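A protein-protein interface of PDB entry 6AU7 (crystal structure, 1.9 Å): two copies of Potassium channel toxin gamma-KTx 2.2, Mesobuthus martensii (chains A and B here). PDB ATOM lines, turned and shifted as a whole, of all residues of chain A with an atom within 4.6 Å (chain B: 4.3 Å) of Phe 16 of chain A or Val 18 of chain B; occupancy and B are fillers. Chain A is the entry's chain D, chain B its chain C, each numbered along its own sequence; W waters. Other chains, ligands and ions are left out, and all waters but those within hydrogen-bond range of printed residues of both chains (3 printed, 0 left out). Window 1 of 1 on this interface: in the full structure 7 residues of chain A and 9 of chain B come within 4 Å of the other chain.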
ATOM      1  N   SER A  12     -12.388  17.349 -21.000  1.00  0.00           N
ATOM      2  CA  SER A  12     -13.493  17.325 -21.959  1.00  0.00           C
ATOM      3  C   SER A  12     -14.893  17.484 -21.342  1.00  0.00           C
ATOM      4  O   SER A  12     -15.758  18.068 -21.992  1.00  0.00           O
ATOM      5  CB  SER A  12     -13.441  16.073 -22.835  1.00  0.00           C
ATOM      6  OG  SER A  12     -12.320  16.149 -23.689  1.00  0.00           O
ATOM      7  N   TYR A  13     -15.106  17.041 -20.095  1.00  0.00           N
ATOM      8  CA  TYR A  13     -16.443  17.192 -19.452  1.00  0.00           C
ATOM      9  C   TYR A  13     -16.903  18.651 -19.426  1.00  0.00           C
ATOM     10  O   TYR A  13     -18.096  18.943 -19.510  1.00  0.00           O
ATOM     11  CB  TYR A  13     -16.463  16.570 -18.010  1.00  0.00           C
ATOM     12  CG  TYR A  13     -15.801  17.463 -16.973  1.00  0.00           C
ATOM     13  CD1 TYR A  13     -16.506  18.539 -16.400  1.00  0.00           C
ATOM     14  CD2 TYR A  13     -14.480  17.233 -16.555  1.00  0.00           C
ATOM     15  CE1 TYR A  13     -15.916  19.371 -15.475  1.00  0.00           C
ATOM     16  CE2 TYR A  13     -13.889  18.060 -15.606  1.00  0.00           C
ATOM     17  CZ  TYR A  13     -14.628  19.130 -15.068  1.00  0.00           C
ATOM     18  OH  TYR A  13     -14.073  19.981 -14.157  1.00  0.00           O
ATOM     19  N   GLN A  14     -15.935  19.569 -19.362  1.00  0.00           N
ATOM     20  CA  GLN A  14     -16.186  21.008 -19.308  1.00  0.00           C
ATOM     21  C   GLN A  14     -16.768  21.559 -20.604  1.00  0.00           C
ATOM     22  O   GLN A  14     -17.383  22.603 -20.595  1.00  0.00           O
ATOM     23  CB  GLN A  14     -14.871  21.734 -19.029  1.00  0.00           C
ATOM     24  CG  GLN A  14     -14.253  21.375 -17.704  1.00  0.00           C
ATOM     25  CD  GLN A  14     -12.844  21.829 -17.540  1.00  0.00           C
ATOM     26  OE1 GLN A  14     -12.190  22.240 -18.492  1.00  0.00           O
ATOM     27  NE2 GLN A  14     -12.334  21.718 -16.326  1.00  0.00           N
ATOM     28  N   CYS A  15     -16.608  20.833 -21.702  1.00  0.00           N
ATOM     29  CA  CYS A  15     -16.979  21.326 -23.012  1.00  0.00           C
ATOM     30  C   CYS A  15     -18.427  21.055 -23.421  1.00  0.00           C
ATOM     31  O   CYS A  15     -18.925  21.613 -24.386  1.00  0.00           O
ATOM     32  CB  CYS A  15     -16.028  20.752 -24.059  1.00  0.00           C
ATOM     33  SG  CYS A  15     -14.357  21.377 -23.839  1.00  0.00           S
ATOM     34  N   PHE A  16     -19.093  20.180 -22.681  1.00  0.00           N
ATOM     35  CA  PHE A  16     -20.426  19.756 -23.094  1.00  0.00           C
ATOM     36  C   PHE A  16     -21.493  20.866 -23.026  1.00  0.00           C
ATOM     37  O   PHE A  16     -22.251  21.033 -23.977  1.00  0.00           O
ATOM     38  CB  PHE A  16     -20.802  18.463 -22.383  1.00  0.00           C
ATOM     39  CG  PHE A  16     -20.142  17.240 -23.005  1.00  0.00           C
ATOM     40  CD1 PHE A  16     -18.842  16.896 -22.665  1.00  0.00           C
ATOM     41  CD2 PHE A  16     -20.786  16.510 -24.023  1.00  0.00           C
ATOM     42  CE1 PHE A  16     -18.197  15.819 -23.326  1.00  0.00           C
ATOM     43  CE2 PHE A  16     -20.183  15.413 -24.588  1.00  0.00           C
ATOM     44  CZ  PHE A  16     -18.885  15.053 -24.240  1.00  0.00           C
ATOM     45  N   PRO A  17     -21.495  21.681 -21.957  1.00  0.00           N
ATOM     46  CA  PRO A  17     -22.480  22.798 -21.931  1.00  0.00           C
ATOM     47  C   PRO A  17     -22.214  23.865 -23.002  1.00  0.00           C
ATOM     48  O   PRO A  17     -23.135  24.360 -23.646  1.00  0.00           O
ATOM     49  CB  PRO A  17     -22.312  23.385 -20.522  1.00  0.00           C
ATOM     50  CG  PRO A  17     -21.758  22.261 -19.720  1.00  0.00           C
ATOM     51  CD  PRO A  17     -20.861  21.476 -20.637  1.00  0.00           C
ATOM     52  N   VAL A  18     -20.951  24.204 -23.188  1.00  0.00           N
ATOM     53  CA  VAL A  18     -20.526  25.133 -24.221  1.00  0.00           C
ATOM     54  C   VAL A  18     -21.009  24.658 -25.604  1.00  0.00           C
ATOM     55  O   VAL A  18     -21.620  25.418 -26.351  1.00  0.00           O
ATOM     56  CB  VAL A  18     -18.968  25.264 -24.270  1.00  0.00           C
ATOM     57  CG1 VAL A  18     -18.622  26.424 -25.195  1.00  0.00           C
ATOM     58  CG2 VAL A  18     -18.364  25.422 -22.855  1.00  0.00           C
ATOM     59  N   CYS A  19     -20.693  23.411 -25.939  1.00  0.00           N
ATOM     60  CA  CYS A  19     -20.973  22.875 -27.273  1.00  0.00           C
ATOM     61  C   CYS A  19     -22.469  22.790 -27.526  1.00  0.00           C
ATOM     62  O   CYS A  19     -22.903  23.095 -28.623  1.00  0.00           O
ATOM     63  CB  CYS A  19     -20.283  21.513 -27.450  1.00  0.00           C
ATOM     64  SG  CYS A  19     -18.477  21.693 -27.504  1.00  0.00           S
ATOM     65  N   LYS A  20     -23.239  22.448 -26.489  1.00  0.00           N
ATOM     66  CA  LYS A  20     -24.696  22.406 -26.554  1.00  0.00           C
ATOM     67  C   LYS A  20     -25.303  23.802 -26.725  1.00  0.00           C
ATOM     68  O   LYS A  20     -26.075  24.041 -27.646  1.00  0.00           O
ATOM     69  CB  LYS A  20     -25.276  21.746 -25.290  1.00  0.00           C
ATOM     70  CG  LYS A  20     -26.710  21.240 -25.438  1.00  0.00           C
ATOM     71  CD  LYS A  20     -26.727  20.002 -26.332  1.00  0.00           C
ATOM     72  CE  LYS A  20     -28.072  19.322 -26.340  1.00  0.00           C
ATOM     73  NZ  LYS A  20     -29.105  20.199 -26.968  1.00  0.00           N
ATOM     74  N   THR A  26     -23.847  17.759 -29.456  1.00  0.00           N
ATOM     75  CA  THR A  26     -23.978  16.856 -28.295  1.00  0.00           C
ATOM     76  C   THR A  26     -22.652  16.182 -27.974  1.00  0.00           C
ATOM     77  O   THR A  26     -22.593  15.344 -27.087  1.00  0.00           O
ATOM     78  CB  THR A  26     -25.067  15.785 -28.511  1.00  0.00           C
ATOM     79  OG1 THR A  26     -24.805  15.111 -29.729  1.00  0.00           O
ATOM     80  CG2 THR A  26     -26.455  16.413 -28.594  1.00  0.00           C
ATOM     81  N   ASN A  27     -21.580  16.565 -28.693  1.00  0.00           N
ATOM     82  CA  ASN A  27     -20.269  16.072 -28.381  1.00  0.00           C
ATOM     83  C   ASN A  27     -19.238  17.215 -28.304  1.00  0.00           C
ATOM     84  O   ASN A  27     -19.266  18.173 -29.099  1.00  0.00           O
ATOM     85  CB  ASN A  27     -19.875  15.025 -29.392  1.00  0.00           C
ATOM     86  CG  ASN A  27     -19.387  13.767 -28.738  1.00  0.00           C
ATOM     87  OD1 ASN A  27     -18.671  13.784 -27.720  1.00  0.00           O
ATOM     88  ND2 ASN A  27     -19.822  12.652 -29.268  1.00  0.00           N
ATOM     89  N   GLY A  28     -18.421  17.158 -27.278  1.00  0.00           N
ATOM     90  CA  GLY A  28     -17.362  18.115 -27.028  1.00  0.00           C
ATOM     91  C   GLY A  28     -16.089  17.360 -26.690  1.00  0.00           C
ATOM     92  O   GLY A  28     -16.134  16.256 -26.147  1.00  0.00           O
ATOM     93  N   ILE B   7     -15.303   9.777 -20.924  1.00  0.00           N
ATOM     94  CA  ILE B   7     -15.052  11.100 -20.397  1.00  0.00           C
ATOM     95  C   ILE B   7     -14.505  10.997 -18.981  1.00  0.00           C
ATOM     96  O   ILE B   7     -15.183  10.513 -18.084  1.00  0.00           O
ATOM     97  CB  ILE B   7     -16.327  11.973 -20.408  1.00  0.00           C
ATOM     98  CG1 ILE B   7     -16.844  12.137 -21.836  1.00  0.00           C
ATOM     99  CG2 ILE B   7     -16.070  13.316 -19.750  1.00  0.00           C
ATOM    100  CD1 ILE B   7     -15.843  12.759 -22.781  1.00  0.00           C
ATOM    101  N   CYS B  15     -20.314  14.971 -14.598  1.00  0.00           N
ATOM    102  CA  CYS B  15     -20.864  14.044 -15.560  1.00  0.00           C
ATOM    103  C   CYS B  15     -22.260  14.430 -16.069  1.00  0.00           C
ATOM    104  O   CYS B  15     -22.729  13.885 -17.051  1.00  0.00           O
ATOM    105  CB  CYS B  15     -20.859  12.666 -14.945  1.00  0.00           C
ATOM    106  SG  CYS B  15     -19.188  12.052 -14.563  1.00  0.00           S
ATOM    107  N   PHE B  16     -22.928  15.364 -15.386  1.00  0.00           N
ATOM    108  CA  PHE B  16     -24.308  15.667 -15.719  1.00  0.00           C
ATOM    109  C   PHE B  16     -24.492  16.297 -17.113  1.00  0.00           C
ATOM    110  O   PHE B  16     -25.386  15.865 -17.836  1.00  0.00           O
ATOM    111  CB  PHE B  16     -24.975  16.513 -14.605  1.00  0.00           C
ATOM    112  CG  PHE B  16     -25.414  15.690 -13.419  1.00  0.00           C
ATOM    113  CD1 PHE B  16     -24.484  15.229 -12.486  1.00  0.00           C
ATOM    114  CD2 PHE B  16     -26.749  15.270 -13.306  1.00  0.00           C
ATOM    115  CE1 PHE B  16     -24.867  14.465 -11.403  1.00  0.00           C
ATOM    116  CE2 PHE B  16     -27.137  14.486 -12.219  1.00  0.00           C
ATOM    117  CZ  PHE B  16     -26.184  14.046 -11.279  1.00  0.00           C
ATOM    118  N   PRO B  17     -23.629  17.237 -17.527  1.00  0.00           N
ATOM    119  CA  PRO B  17     -23.803  17.783 -18.903  1.00  0.00           C
ATOM    120  C   PRO B  17     -23.530  16.741 -20.000  1.00  0.00           C
ATOM    121  O   PRO B  17     -24.278  16.667 -20.989  1.00  0.00           O
ATOM    122  CB  PRO B  17     -22.776  18.918 -18.973  1.00  0.00           C
ATOM    123  CG  PRO B  17     -22.551  19.320 -17.551  1.00  0.00           C
ATOM    124  CD  PRO B  17     -22.712  18.055 -16.716  1.00  0.00           C
ATOM    125  N   VAL B  18     -22.474  15.949 -19.821  1.00  0.00           N
ATOM    126  CA  VAL B  18     -22.168  14.899 -20.784  1.00  0.00           C
ATOM    127  C   VAL B  18     -23.321  13.913 -20.911  1.00  0.00           C
ATOM    128  O   VAL B  18     -23.743  13.596 -22.032  1.00  0.00           O
ATOM    129  CB  VAL B  18     -20.862  14.140 -20.558  1.00  0.00           C
ATOM    130  CG1 VAL B  18     -20.820  13.396 -19.275  1.00  0.00           C
ATOM    131  CG2 VAL B  18     -20.678  13.157 -21.695  1.00  0.00           C
ATOM    132  N   CYS B  19     -23.844  13.459 -19.780  1.00  0.00           N
ATOM    133  CA  CYS B  19     -24.898  12.436 -19.790  1.00  0.00           C
ATOM    134  C   CYS B  19     -26.187  12.941 -20.401  1.00  0.00           C
ATOM    135  O   CYS B  19     -26.825  12.221 -21.157  1.00  0.00           O
ATOM    136  CB  CYS B  19     -25.097  11.927 -18.366  1.00  0.00           C
ATOM    137  SG  CYS B  19     -23.606  11.011 -17.817  1.00  0.00           S
ATOM    138  N   LYS B  20     -26.500  14.220 -20.148  1.00  0.00           N
ATOM    139  CA  LYS B  20     -27.668  14.887 -20.732  1.00  0.00           C
ATOM    140  C   LYS B  20     -27.508  15.064 -22.253  1.00  0.00           C
ATOM    141  O   LYS B  20     -28.369  14.662 -23.027  1.00  0.00           O
ATOM    142  CB  LYS B  20     -27.883  16.259 -20.064  1.00  0.00           C
ATOM    143  CG  LYS B  20     -29.252  16.860 -20.265  1.00  0.00           C
ATOM    144  CD  LYS B  20     -30.331  16.063 -19.511  1.00  0.00           C
ATOM    145  CE  LYS B  20     -31.683  16.730 -19.660  1.00  0.00           C
ATOM    146  NZ  LYS B  20     -32.150  16.799 -21.078  1.00  0.00           N
ATOM    147  N   SER B  21     -26.380  15.659 -22.657  1.00  0.00           N
ATOM    148  CA  SER B  21     -26.112  15.957 -24.058  1.00  0.00           C
ATOM    149  C   SER B  21     -26.076  14.694 -24.936  1.00  0.00           C
ATOM    150  O   SER B  21     -26.722  14.648 -25.980  1.00  0.00           O
ATOM    151  CB  SER B  21     -24.760  16.710 -24.220  1.00  0.00           C
ATOM    152  OG  SER B  21     -24.836  18.058 -23.813  1.00  0.00           O
ATOM    153  N   ARG B  22     -25.300  13.702 -24.520  1.00  0.00           N
ATOM    154  CA  ARG B  22     -25.013  12.557 -25.374  1.00  0.00           C
ATOM    155  C   ARG B  22     -26.177  11.587 -25.402  1.00  0.00           C
ATOM    156  O   ARG B  22     -26.397  10.949 -26.425  1.00  0.00           O
ATOM    157  CB  ARG B  22     -23.769  11.774 -24.900  1.00  0.00           C
ATOM    158  CG  ARG B  22     -22.507  11.982 -25.773  1.00  0.00           C
ATOM    159  CD  ARG B  22     -21.544  10.831 -25.584  1.00  0.00           C
ATOM    160  NE  ARG B  22     -20.156  11.223 -25.822  1.00  0.00           N
ATOM    161  CZ  ARG B  22     -19.096  10.457 -25.581  1.00  0.00           C
ATOM    162  NH1 ARG B  22     -17.877  10.916 -25.843  1.00  0.00           N
ATOM    163  NH2 ARG B  22     -19.216   9.219 -25.102  1.00  0.00           N
ATOM    164  N   CYS B  35     -17.078   9.031 -16.472  1.00  0.00           N
ATOM    165  CA  CYS B  35     -18.522   9.279 -16.398  1.00  0.00           C
ATOM    166  C   CYS B  35     -19.365   8.080 -16.869  1.00  0.00           C
ATOM    167  O   CYS B  35     -19.120   7.490 -17.938  1.00  0.00           O
ATOM    168  CB  CYS B  35     -18.924  10.528 -17.171  1.00  0.00           C
ATOM    169  SG  CYS B  35     -18.314  12.031 -16.409  1.00  0.00           S
HETATM  170  O   HOH W   1     -16.133  13.301 -26.874  1.00  0.00           O
HETATM  171  O   HOH W   2     -19.953  16.722 -18.728  1.00  0.00           O
HETATM  172  O   HOH W   3     -22.942  19.088 -25.663  1.00  0.00           O
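Phe 16 of chain A touches Pro 17 of chain B, but with the chains exchanged Pro 17 of chain A does not touch Phe 16 of chain B (7.1 Å).
Phe 16 of chain A touches Val 18 of chain B, but with the chains exchanged Val 18 of chain A does not touch Phe 16 of chain B (10.6 Å).
Pro 17 of chain A touches its own counterpart, Pro 17 of chain B.
Positions printed for both chains: 15, 16, 17, 18, 19 and 20.
Of the 10 pairs that touch across the chains among the printed residues, 1 has its exchanged pair printed and touching as well.
Tyr 13 of chain A touches Ile 7 of chain B (CB to CG2, 3.7 Å).
CE1 of Phe 16 of chain A touches CD1 of Ile 7 of chain B, at 3.9 Å.
Phe 16 of chain A touches Pro 17 of chain B.
Val 18 of chain B touches Phe 16 of chain A (CG2 to CZ, 3.6 Å).
OG of Ser 21 of chain B touches O of Phe 16 of chain A (3.9 Å).
CG of Pro 17 of chain A touches CB of Pro 17 of chain B, at 3.6 Å.
Ser 21 of chain B touches Lys 20 of chain A (OG to CD, 3.7 Å).
Ser 21 of chain B touches Thr 26 of chain A.
Arg 22 of chain B touches Thr 26 of chain A (CG to O, 3.6 Å).
Asn 27 of chain A touches Arg 22 of chain B.
O of Ile 7 of chain B lies within hydrogen-bond range of N of Cys 35 of chain B (2.9 Å).
OG of Ser 21 of chain B is in hydrogen-bond range of O of Pro 17 of chain B.
The side-chain amide nitrogen (NE2) of Gln 14 of chain A sits at hydrogen-bond distance from the side-chain hydroxyl (OH) of Tyr 13 of chain A (3.3 Å).
The side-chain sulfur (SG) of Cys 15 of chain B is disulfide-bonded to the side-chain sulfur (SG) of Cys 35 of chain B.
Printed residues of chain A that touch a printed residue of chain B: Tyr 13, Phe 16, Pro 17, Lys 20, Thr 26 and Asn 27.
Hydrophobic or aromatic side chains of chain A that line the printed part of chain B: Tyr 13, Phe 16 and Pro 17.
Among the printed residues, 10 pairs touch across the chains.
Among the printed residues, no Asp or Glu carboxylate lies within 4 Å of a Lys or Arg side-chain nitrogen of the other chain.
Water W3 lies within hydrogen-bond range of the backbone carbonyl oxygen (O) of Phe 16 of chain A, the side-chain hydroxyl (OG) of Ser 21 of chain B and the backbone NH (N) of Lys 20 of chain A.
Water W1 lies within hydrogen-bond range of OD1 of Asn 27 of chain A, O of Gly 28 of chain A and NH1 of Arg 22 of chain B.
Water W2 lies within hydrogen-bond range of N of Val 18 of chain B (2.9 Å) and O of Tyr 13 of chain A (3.0 Å).
Of the printed residues of chain B, Tyr 13 of chain A touches Ile 7 (3.7 Å).
Cys 15 of chain A touches none of the printed residues of chain B.
Phe 16 of chain A touches just these residues of chain B: Ile 7 (3.9 Å), Pro 17 (3.97 Å), Val 18 (3.6 Å) and Ser 21 (3.9 Å).
Of the printed residues of chain B, Lys 20 of chain A touches Ser 21.
Val 18 of chain B touches just one residue of chain A: Phe 16.
The nearest printed residue of chain B that does not touch Phe 16 of chain A is Arg 22 of chain B (4.3 Å).
The nearest printed residue of chain A that does not touch Val 18 of chain B is Tyr 13 of chain A (5.3 Å).
The nearest printed residue of chain B that does not touch Asn 27 of chain A is Ser 21 of chain B (5.5 Å).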
